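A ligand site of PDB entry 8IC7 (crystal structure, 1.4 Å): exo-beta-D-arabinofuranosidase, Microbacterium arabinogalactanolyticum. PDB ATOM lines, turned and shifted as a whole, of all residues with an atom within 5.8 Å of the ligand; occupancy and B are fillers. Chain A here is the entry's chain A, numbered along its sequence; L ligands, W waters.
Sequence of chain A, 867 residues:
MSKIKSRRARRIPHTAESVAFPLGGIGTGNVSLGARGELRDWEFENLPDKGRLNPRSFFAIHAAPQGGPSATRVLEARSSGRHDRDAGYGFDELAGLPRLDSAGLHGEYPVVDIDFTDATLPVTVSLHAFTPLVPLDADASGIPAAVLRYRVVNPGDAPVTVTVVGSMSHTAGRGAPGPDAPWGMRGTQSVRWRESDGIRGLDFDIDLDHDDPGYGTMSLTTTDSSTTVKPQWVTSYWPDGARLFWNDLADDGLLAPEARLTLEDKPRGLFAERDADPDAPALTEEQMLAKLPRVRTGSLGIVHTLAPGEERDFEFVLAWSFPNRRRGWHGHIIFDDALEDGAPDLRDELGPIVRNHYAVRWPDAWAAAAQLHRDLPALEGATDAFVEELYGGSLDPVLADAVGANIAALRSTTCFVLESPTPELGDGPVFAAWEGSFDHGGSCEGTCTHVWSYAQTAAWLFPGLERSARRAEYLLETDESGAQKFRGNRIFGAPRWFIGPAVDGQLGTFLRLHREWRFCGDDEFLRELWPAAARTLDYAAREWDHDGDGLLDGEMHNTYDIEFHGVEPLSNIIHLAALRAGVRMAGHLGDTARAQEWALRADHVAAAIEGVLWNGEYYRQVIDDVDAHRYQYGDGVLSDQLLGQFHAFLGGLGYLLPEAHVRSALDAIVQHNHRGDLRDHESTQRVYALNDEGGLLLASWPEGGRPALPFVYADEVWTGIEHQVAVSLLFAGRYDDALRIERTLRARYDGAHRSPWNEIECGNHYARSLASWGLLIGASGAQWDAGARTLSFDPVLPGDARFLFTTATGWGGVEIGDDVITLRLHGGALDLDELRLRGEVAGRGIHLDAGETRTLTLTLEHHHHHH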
ATOM      1  N   GLU A 435      -3.371  18.001  16.264  1.00  0.00           N
ATOM      2  CA  GLU A 435      -3.358  19.120  17.200  1.00  0.00           C
ATOM      3  C   GLU A 435      -4.213  20.256  16.642  1.00  0.00           C
ATOM      4  O   GLU A 435      -4.796  21.035  17.396  1.00  0.00           O
ATOM      5  CB  GLU A 435      -1.989  19.675  17.472  1.00  0.00           C
ATOM      6  CG  GLU A 435      -1.048  18.676  18.125  1.00  0.00           C
ATOM      7  CD  GLU A 435       0.388  19.105  18.238  1.00  0.00           C
ATOM      8  OE1 GLU A 435       0.699  20.300  18.000  1.00  0.00           O
ATOM      9  OE2 GLU A 435       1.238  18.199  18.528  1.00  0.00           O
ATOM     10  N   CYS A 444       0.189  18.122  12.943  1.00  0.00           N
ATOM     11  CA  CYS A 444       0.807  17.458  14.079  1.00  0.00           C
ATOM     12  C   CYS A 444      -0.062  16.294  14.574  1.00  0.00           C
ATOM     13  O   CYS A 444      -0.829  16.391  15.543  1.00  0.00           O
ATOM     14  CB  CYS A 444       1.127  18.485  15.180  1.00  0.00           C
ATOM     15  SG  CYS A 444       2.287  19.762  14.668  1.00  0.00           S
ATOM     16  N   CYS A 448      -1.847  13.982  20.003  1.00  0.00           N
ATOM     17  CA  CYS A 448      -0.716  14.355  20.809  1.00  0.00           C
ATOM     18  C   CYS A 448      -1.046  14.599  22.280  1.00  0.00           C
ATOM     19  O   CYS A 448      -1.890  15.412  22.588  1.00  0.00           O
ATOM     20  CB  CYS A 448      -0.091  15.588  20.245  1.00  0.00           C
ATOM     21  SG  CYS A 448       1.329  16.158  21.171  1.00  0.00           S
ATOM     22  N   HIS A 450       0.642  15.720  24.981  1.00  0.00           N
ATOM     23  CA  HIS A 450       1.024  16.919  25.692  1.00  0.00           C
ATOM     24  C   HIS A 450       0.122  18.095  25.315  1.00  0.00           C
ATOM     25  O   HIS A 450      -0.130  18.964  26.145  1.00  0.00           O
ATOM     26  CB  HIS A 450       2.524  17.225  25.664  1.00  0.00           C
ATOM     27  CG  HIS A 450       3.194  17.435  24.367  1.00  0.00           C
ATOM     28  ND1 HIS A 450       2.744  18.402  23.488  1.00  0.00           N
ATOM     29  CD2 HIS A 450       4.238  16.800  23.779  1.00  0.00           C
ATOM     30  CE1 HIS A 450       3.574  18.409  22.453  1.00  0.00           C
ATOM     31  NE2 HIS A 450       4.453  17.409  22.562  1.00  0.00           N
ATOM     32  N   VAL A 451      -0.405  18.104  24.096  1.00  0.00           N
ATOM     33  CA  VAL A 451      -1.402  19.112  23.691  1.00  0.00           C
ATOM     34  C   VAL A 451      -2.807  18.812  24.184  1.00  0.00           C
ATOM     35  O   VAL A 451      -3.497  19.656  24.785  1.00  0.00           O
ATOM     36  CB  VAL A 451      -1.351  19.325  22.165  1.00  0.00           C
ATOM     37  CG1 VAL A 451      -2.462  20.272  21.737  1.00  0.00           C
ATOM     38  CG2 VAL A 451       0.023  19.821  21.728  1.00  0.00           C
ATOM     39  N   PHE A 486       3.847   9.866  23.070  1.00  0.00           N
ATOM     40  CA  PHE A 486       2.973  11.050  23.119  1.00  0.00           C
ATOM     41  C   PHE A 486       2.347  11.382  21.754  1.00  0.00           C
ATOM     42  O   PHE A 486       1.481  12.242  21.657  1.00  0.00           O
ATOM     43  CB  PHE A 486       3.688  12.256  23.729  1.00  0.00           C
ATOM     44  CG  PHE A 486       4.826  12.888  22.962  1.00  0.00           C
ATOM     45  CD1 PHE A 486       4.567  13.816  21.941  1.00  0.00           C
ATOM     46  CD2 PHE A 486       6.137  12.629  23.288  1.00  0.00           C
ATOM     47  CE1 PHE A 486       5.610  14.454  21.274  1.00  0.00           C
ATOM     48  CE2 PHE A 486       7.173  13.282  22.648  1.00  0.00           C
ATOM     49  CZ  PHE A 486       6.906  14.177  21.644  1.00  0.00           C
ATOM     50  N   ARG A 487       2.709  10.640  20.736  1.00  0.00           N
ATOM     51  CA  ARG A 487       1.963  10.621  19.472  1.00  0.00           C
ATOM     52  C   ARG A 487       1.702   9.181  19.078  1.00  0.00           C
ATOM     53  O   ARG A 487       2.617   8.363  19.080  1.00  0.00           O
ATOM     54  CB  ARG A 487       2.698  11.303  18.310  1.00  0.00           C
ATOM     55  CG  ARG A 487       3.046  12.754  18.590  1.00  0.00           C
ATOM     56  CD  ARG A 487       3.661  13.456  17.386  1.00  0.00           C
ATOM     57  NE  ARG A 487       4.084  14.823  17.684  1.00  0.00           N
ATOM     58  CZ  ARG A 487       3.267  15.865  17.781  1.00  0.00           C
ATOM     59  NH1 ARG A 487       2.006  15.751  17.429  1.00  0.00           N
ATOM     60  NH2 ARG A 487       3.718  17.027  18.241  1.00  0.00           N
ATOM     61  N   THR A 559       5.710  20.069  25.934  1.00  0.00           N
ATOM     62  CA  THR A 559       4.883  20.634  24.884  1.00  0.00           C
ATOM     63  C   THR A 559       5.575  21.785  24.161  1.00  0.00           C
ATOM     64  O   THR A 559       5.086  22.251  23.117  1.00  0.00           O
ATOM     65  CB  THR A 559       3.525  21.025  25.472  1.00  0.00           C
ATOM     66  OG1 THR A 559       2.574  21.074  24.393  1.00  0.00           O
ATOM     67  CG2 THR A 559       3.519  22.328  26.242  1.00  0.00           C
ATOM     68  N   TYR A 560       6.648  22.334  24.756  1.00  0.00           N
ATOM     69  CA  TYR A 560       7.360  23.419  24.091  1.00  0.00           C
ATOM     70  C   TYR A 560       8.343  22.863  23.075  1.00  0.00           C
ATOM     71  O   TYR A 560       9.160  23.636  22.544  1.00  0.00           O
ATOM     72  CB  TYR A 560       8.035  24.342  25.108  1.00  0.00           C
ATOM     73  CG  TYR A 560       7.129  24.828  26.190  1.00  0.00           C
ATOM     74  CD1 TYR A 560       5.895  25.360  25.887  1.00  0.00           C
ATOM     75  CD2 TYR A 560       7.500  24.743  27.529  1.00  0.00           C
ATOM     76  CE1 TYR A 560       5.051  25.860  26.872  1.00  0.00           C
ATOM     77  CE2 TYR A 560       6.620  25.136  28.521  1.00  0.00           C
ATOM     78  CZ  TYR A 560       5.427  25.743  28.208  1.00  0.00           C
ATOM     79  OH  TYR A 560       4.590  26.186  29.185  1.00  0.00           O
ATOM     80  N   ASP A 561       8.314  21.556  22.797  1.00  0.00           N
ATOM     81  CA  ASP A 561       9.119  20.934  21.730  1.00  0.00           C
ATOM     82  C   ASP A 561      10.622  20.945  22.035  1.00  0.00           C
ATOM     83  O   ASP A 561      11.428  20.627  21.150  1.00  0.00           O
ATOM     84  CB  ASP A 561       8.827  21.541  20.362  1.00  0.00           C
ATOM     85  CG  ASP A 561       7.433  21.253  19.863  1.00  0.00           C
ATOM     86  OD1 ASP A 561       6.888  20.146  20.163  1.00  0.00           O
ATOM     87  OD2 ASP A 561       6.892  22.127  19.095  1.00  0.00           O
ATOM     88  N   ARG A 686       6.746  33.021  16.882  1.00  0.00           N
ATOM     89  CA  ARG A 686       5.549  33.055  16.052  1.00  0.00           C
ATOM     90  C   ARG A 686       4.551  34.005  16.661  1.00  0.00           C
ATOM     91  O   ARG A 686       4.566  34.220  17.885  1.00  0.00           O
ATOM     92  CB  ARG A 686       4.885  31.671  15.941  1.00  0.00           C
ATOM     93  CG  ARG A 686       5.832  30.640  15.375  1.00  0.00           C
ATOM     94  CD  ARG A 686       5.332  29.200  15.557  1.00  0.00           C
ATOM     95  NE  ARG A 686       5.195  28.852  16.955  1.00  0.00           N
ATOM     96  CZ  ARG A 686       4.401  27.879  17.388  1.00  0.00           C
ATOM     97  NH1 ARG A 686       3.974  26.914  16.569  1.00  0.00           N
ATOM     98  NH2 ARG A 686       4.098  27.852  18.664  1.00  0.00           N
ATOM     99  N   TYR A 688       0.628  35.132  17.474  1.00  0.00           N
ATOM    100  CA  TYR A 688      -0.792  34.878  17.708  1.00  0.00           C
ATOM    101  C   TYR A 688      -1.490  36.049  18.423  1.00  0.00           C
ATOM    102  O   TYR A 688      -2.634  35.950  18.816  1.00  0.00           O
ATOM    103  CB  TYR A 688      -0.944  33.596  18.543  1.00  0.00           C
ATOM    104  CG  TYR A 688      -0.165  32.455  17.956  1.00  0.00           C
ATOM    105  CD1 TYR A 688      -0.564  31.818  16.791  1.00  0.00           C
ATOM    106  CD2 TYR A 688       0.992  31.997  18.532  1.00  0.00           C
ATOM    107  CE1 TYR A 688       0.152  30.803  16.231  1.00  0.00           C
ATOM    108  CE2 TYR A 688       1.718  30.938  18.003  1.00  0.00           C
ATOM    109  CZ  TYR A 688       1.301  30.336  16.828  1.00  0.00           C
ATOM    110  OH  TYR A 688       2.016  29.371  16.246  1.00  0.00           O
ATOM    111  N   TYR A 713       9.241  29.257  22.380  1.00  0.00           N
ATOM    112  CA  TYR A 713       7.885  29.819  22.312  1.00  0.00           C
ATOM    113  C   TYR A 713       7.616  30.749  23.509  1.00  0.00           C
ATOM    114  O   TYR A 713       6.516  31.274  23.680  1.00  0.00           O
ATOM    115  CB  TYR A 713       6.849  28.683  22.335  1.00  0.00           C
ATOM    116  CG  TYR A 713       7.025  27.594  21.304  1.00  0.00           C
ATOM    117  CD1 TYR A 713       7.197  27.912  19.979  1.00  0.00           C
ATOM    118  CD2 TYR A 713       6.921  26.245  21.655  1.00  0.00           C
ATOM    119  CE1 TYR A 713       7.318  26.929  19.011  1.00  0.00           C
ATOM    120  CE2 TYR A 713       6.999  25.257  20.703  1.00  0.00           C
ATOM    121  CZ  TYR A 713       7.204  25.577  19.371  1.00  0.00           C
ATOM    122  OH  TYR A 713       7.283  24.612  18.414  1.00  0.00           O
ATOM    123  N   GLU A 716       5.714  33.987  22.973  1.00  0.00           N
ATOM    124  CA  GLU A 716       4.455  33.846  22.276  1.00  0.00           C
ATOM    125  C   GLU A 716       3.285  33.923  23.256  1.00  0.00           C
ATOM    126  O   GLU A 716       3.478  33.980  24.468  1.00  0.00           O
ATOM    127  CB  GLU A 716       4.398  32.509  21.536  1.00  0.00           C
ATOM    128  CG  GLU A 716       5.513  32.345  20.505  1.00  0.00           C
ATOM    129  CD  GLU A 716       5.495  31.046  19.710  1.00  0.00           C
ATOM    130  OE1 GLU A 716       4.678  30.194  20.042  1.00  0.00           O
ATOM    131  OE2 GLU A 716       6.234  30.941  18.718  1.00  0.00           O
ATOM    132  N   TRP A 718      -0.373  31.747  23.686  1.00  0.00           N
ATOM    133  CA  TRP A 718      -1.186  30.610  23.326  1.00  0.00           C
ATOM    134  C   TRP A 718      -2.514  30.708  24.043  1.00  0.00           C
ATOM    135  O   TRP A 718      -2.550  30.753  25.278  1.00  0.00           O
ATOM    136  CB  TRP A 718      -0.499  29.306  23.701  1.00  0.00           C
ATOM    137  CG  TRP A 718       0.765  29.025  22.974  1.00  0.00           C
ATOM    138  CD1 TRP A 718       1.408  29.767  22.023  1.00  0.00           C
ATOM    139  CD2 TRP A 718       1.576  27.841  23.154  1.00  0.00           C
ATOM    140  NE1 TRP A 718       2.529  29.146  21.597  1.00  0.00           N
ATOM    141  CE2 TRP A 718       2.682  27.957  22.278  1.00  0.00           C
ATOM    142  CE3 TRP A 718       1.463  26.686  23.967  1.00  0.00           C
ATOM    143  CZ2 TRP A 718       3.661  26.970  22.181  1.00  0.00           C
ATOM    144  CZ3 TRP A 718       2.470  25.754  23.893  1.00  0.00           C
ATOM    145  CH2 TRP A 718       3.536  25.883  23.008  1.00  0.00           C
ATOM    146  N   GLU A 761      -3.081  28.156  16.943  1.00  0.00           N
ATOM    147  CA  GLU A 761      -1.732  28.035  17.452  1.00  0.00           C
ATOM    148  C   GLU A 761      -0.977  27.337  16.322  1.00  0.00           C
ATOM    149  O   GLU A 761      -0.827  27.958  15.259  1.00  0.00           O
ATOM    150  CB  GLU A 761      -1.648  27.309  18.797  1.00  0.00           C
ATOM    151  CG  GLU A 761      -0.332  27.470  19.508  1.00  0.00           C
ATOM    152  CD  GLU A 761      -0.187  26.411  20.583  1.00  0.00           C
ATOM    153  OE1 GLU A 761      -1.002  26.447  21.538  1.00  0.00           O
ATOM    154  OE2 GLU A 761       0.679  25.520  20.449  1.00  0.00           O
ATOM    155  N   CYS A 762      -0.490  26.091  16.472  1.00  0.00           N
ATOM    156  CA  CYS A 762       0.105  25.378  15.365  1.00  0.00           C
ATOM    157  C   CYS A 762      -1.016  24.734  14.558  1.00  0.00           C
ATOM    158  O   CYS A 762      -1.227  23.533  14.562  1.00  0.00           O
ATOM    159  CB  CYS A 762       1.153  24.377  15.827  1.00  0.00           C
ATOM    160  SG  CYS A 762       2.120  23.855  14.389  1.00  0.00           S
ATOM    161  N   TYR A 766      -7.290  24.785  17.050  1.00  0.00           N
ATOM    162  CA  TYR A 766      -6.213  24.162  17.786  1.00  0.00           C
ATOM    163  C   TYR A 766      -6.760  23.500  19.062  1.00  0.00           C
ATOM    164  O   TYR A 766      -7.490  24.096  19.866  1.00  0.00           O
ATOM    165  CB  TYR A 766      -5.097  25.185  18.077  1.00  0.00           C
ATOM    166  CG  TYR A 766      -3.808  24.474  18.385  1.00  0.00           C
ATOM    167  CD1 TYR A 766      -3.079  23.845  17.381  1.00  0.00           C
ATOM    168  CD2 TYR A 766      -3.343  24.425  19.687  1.00  0.00           C
ATOM    169  CE1 TYR A 766      -1.940  23.120  17.693  1.00  0.00           C
ATOM    170  CE2 TYR A 766      -2.211  23.694  19.988  1.00  0.00           C
ATOM    171  CZ  TYR A 766      -1.502  23.059  19.004  1.00  0.00           C
ATOM    172  OH  TYR A 766      -0.397  22.332  19.363  1.00  0.00           O
ATOM    173  N   ARG A 768      -5.542  22.825  21.933  1.00  0.00           N
ATOM    174  CA  ARG A 768      -5.229  23.425  23.239  1.00  0.00           C
ATOM    175  C   ARG A 768      -6.334  24.424  23.637  1.00  0.00           C
ATOM    176  O   ARG A 768      -6.579  24.649  24.814  1.00  0.00           O
ATOM    177  CB  ARG A 768      -3.876  24.121  23.220  1.00  0.00           C
ATOM    178  CG  ARG A 768      -3.091  23.855  24.509  1.00  0.00           C
ATOM    179  CD  ARG A 768      -1.856  24.693  24.588  1.00  0.00           C
ATOM    180  NE  ARG A 768      -0.949  24.481  23.457  1.00  0.00           N
ATOM    181  CZ  ARG A 768       0.002  23.526  23.400  1.00  0.00           C
ATOM    182  NH1 ARG A 768       0.132  22.638  24.374  1.00  0.00           N
ATOM    183  NH2 ARG A 768       0.797  23.445  22.359  1.00  0.00           N
HETATM  184  O1  LIG L   1       4.356  19.592  19.620  1.00  0.00           O
HETATM  185  C1  LIG L   1       3.464  20.650  19.332  1.00  0.00           C
HETATM  186  C2  LIG L   1       3.715  21.221  17.921  1.00  0.00           C
HETATM  187  O2  LIG L   1       3.210  22.560  18.007  1.00  0.00           O
HETATM  188  C3  LIG L   1       3.649  21.901  20.201  1.00  0.00           C
HETATM  189  O3  LIG L   1       3.072  21.752  21.476  1.00  0.00           O
HETATM  190  C4  LIG L   1       2.918  22.960  19.356  1.00  0.00           C
HETATM  191  C5  LIG L   1       3.458  24.362  19.621  1.00  0.00           C
HETATM  192  O4  LIG L   1       2.704  25.326  18.887  1.00  0.00           O
HETATM  193  O5  LIG L   1       5.039  21.206  17.505  1.00  0.00           O
HETATM  194  O   HOH W   1       5.292  22.662  15.243  1.00  0.00           O
HETATM  195  O   HOH W   2       6.023  18.783  16.615  1.00  0.00           O
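An oxygen (O4) of the ligand is in hydrogen-bond range of the side-chain carboxylate of Glu 761 (2.6 Å).
OD2 of Asp 561 sits at hydrogen-bond distance from O5 of the ligand.
O of Thr 559 is in hydrogen-bond range of O3 of the ligand (2.6 Å).
An oxygen (O3) of the ligand lies within hydrogen-bond range of the side-chain hydroxyl of Thr 559, at 3.0 Å.
NH2 of Arg 686 lies within hydrogen-bond range of O4 of the ligand, at 2.9 Å.
O3 of the ligand sits at hydrogen-bond distance from NH2 of Arg 768 (3.0 Å).
An oxygen (O1) of the ligand lies within hydrogen-bond range of the guanidinium group (NH2) of Arg 487, 3.0 Å away.
The side-chain carboxylate of Glu 761 is in salt-bridge range of the guanidinium group of Arg 768, 2.7 Å away.
OH of Tyr 713 lies within hydrogen-bond range of OD2 of Asp 561 (2.6 Å).
The side-chain hydroxyl of Thr 559 lies within hydrogen-bond range of the guanidinium group of Arg 768, 2.9 Å away.
OH of Tyr 688 lies close to NH1 of Arg 686 (3.2 Å).
O of Cys 444 sits at hydrogen-bond distance from NH1 of Arg 487 (3.5 Å).
N of Glu 435 lies within hydrogen-bond range of O of Cys 444.
The side-chain carboxylate of Glu 435 is in hydrogen-bond range of the side-chain sulfur of Cys 448.
The indole nitrogen (NE1) of Trp 718 is in hydrogen-bond range of the side-chain carboxylate (OE1) of Glu 716 (2.9 Å).
O2 of the ligand sits close to OE1 of Glu 435, 3.4 Å away.
Cys 444 touches the ligand (SG to C2, 3.8 Å).
His 450 touches the ligand.
Val 451 touches the ligand.
Tyr 713 touches the ligand (CE2 to C5, 3.8 Å).
Trp 718 touches the ligand.
Cys 762 touches the ligand (CB to O2, 3.5 Å).
Tyr 766 touches the ligand (OH to C4, 3.4 Å).
14 residues have an atom within 4 Å of the ligand: Glu 435, Cys 444, His 450, Val 451, Arg 487, Thr 559, Asp 561, Arg 686, Tyr 713, Trp 718, Glu 761, Cys 762, Tyr 766 and Arg 768.
Water W1 bridges an oxygen (O5) of the ligand (2.7 Å) and the side-chain sulfur (SG) of Cys 762 (3.5 Å).
Water W2 lies within hydrogen-bond range of O5 of the ligand and NH2 of Arg 487.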
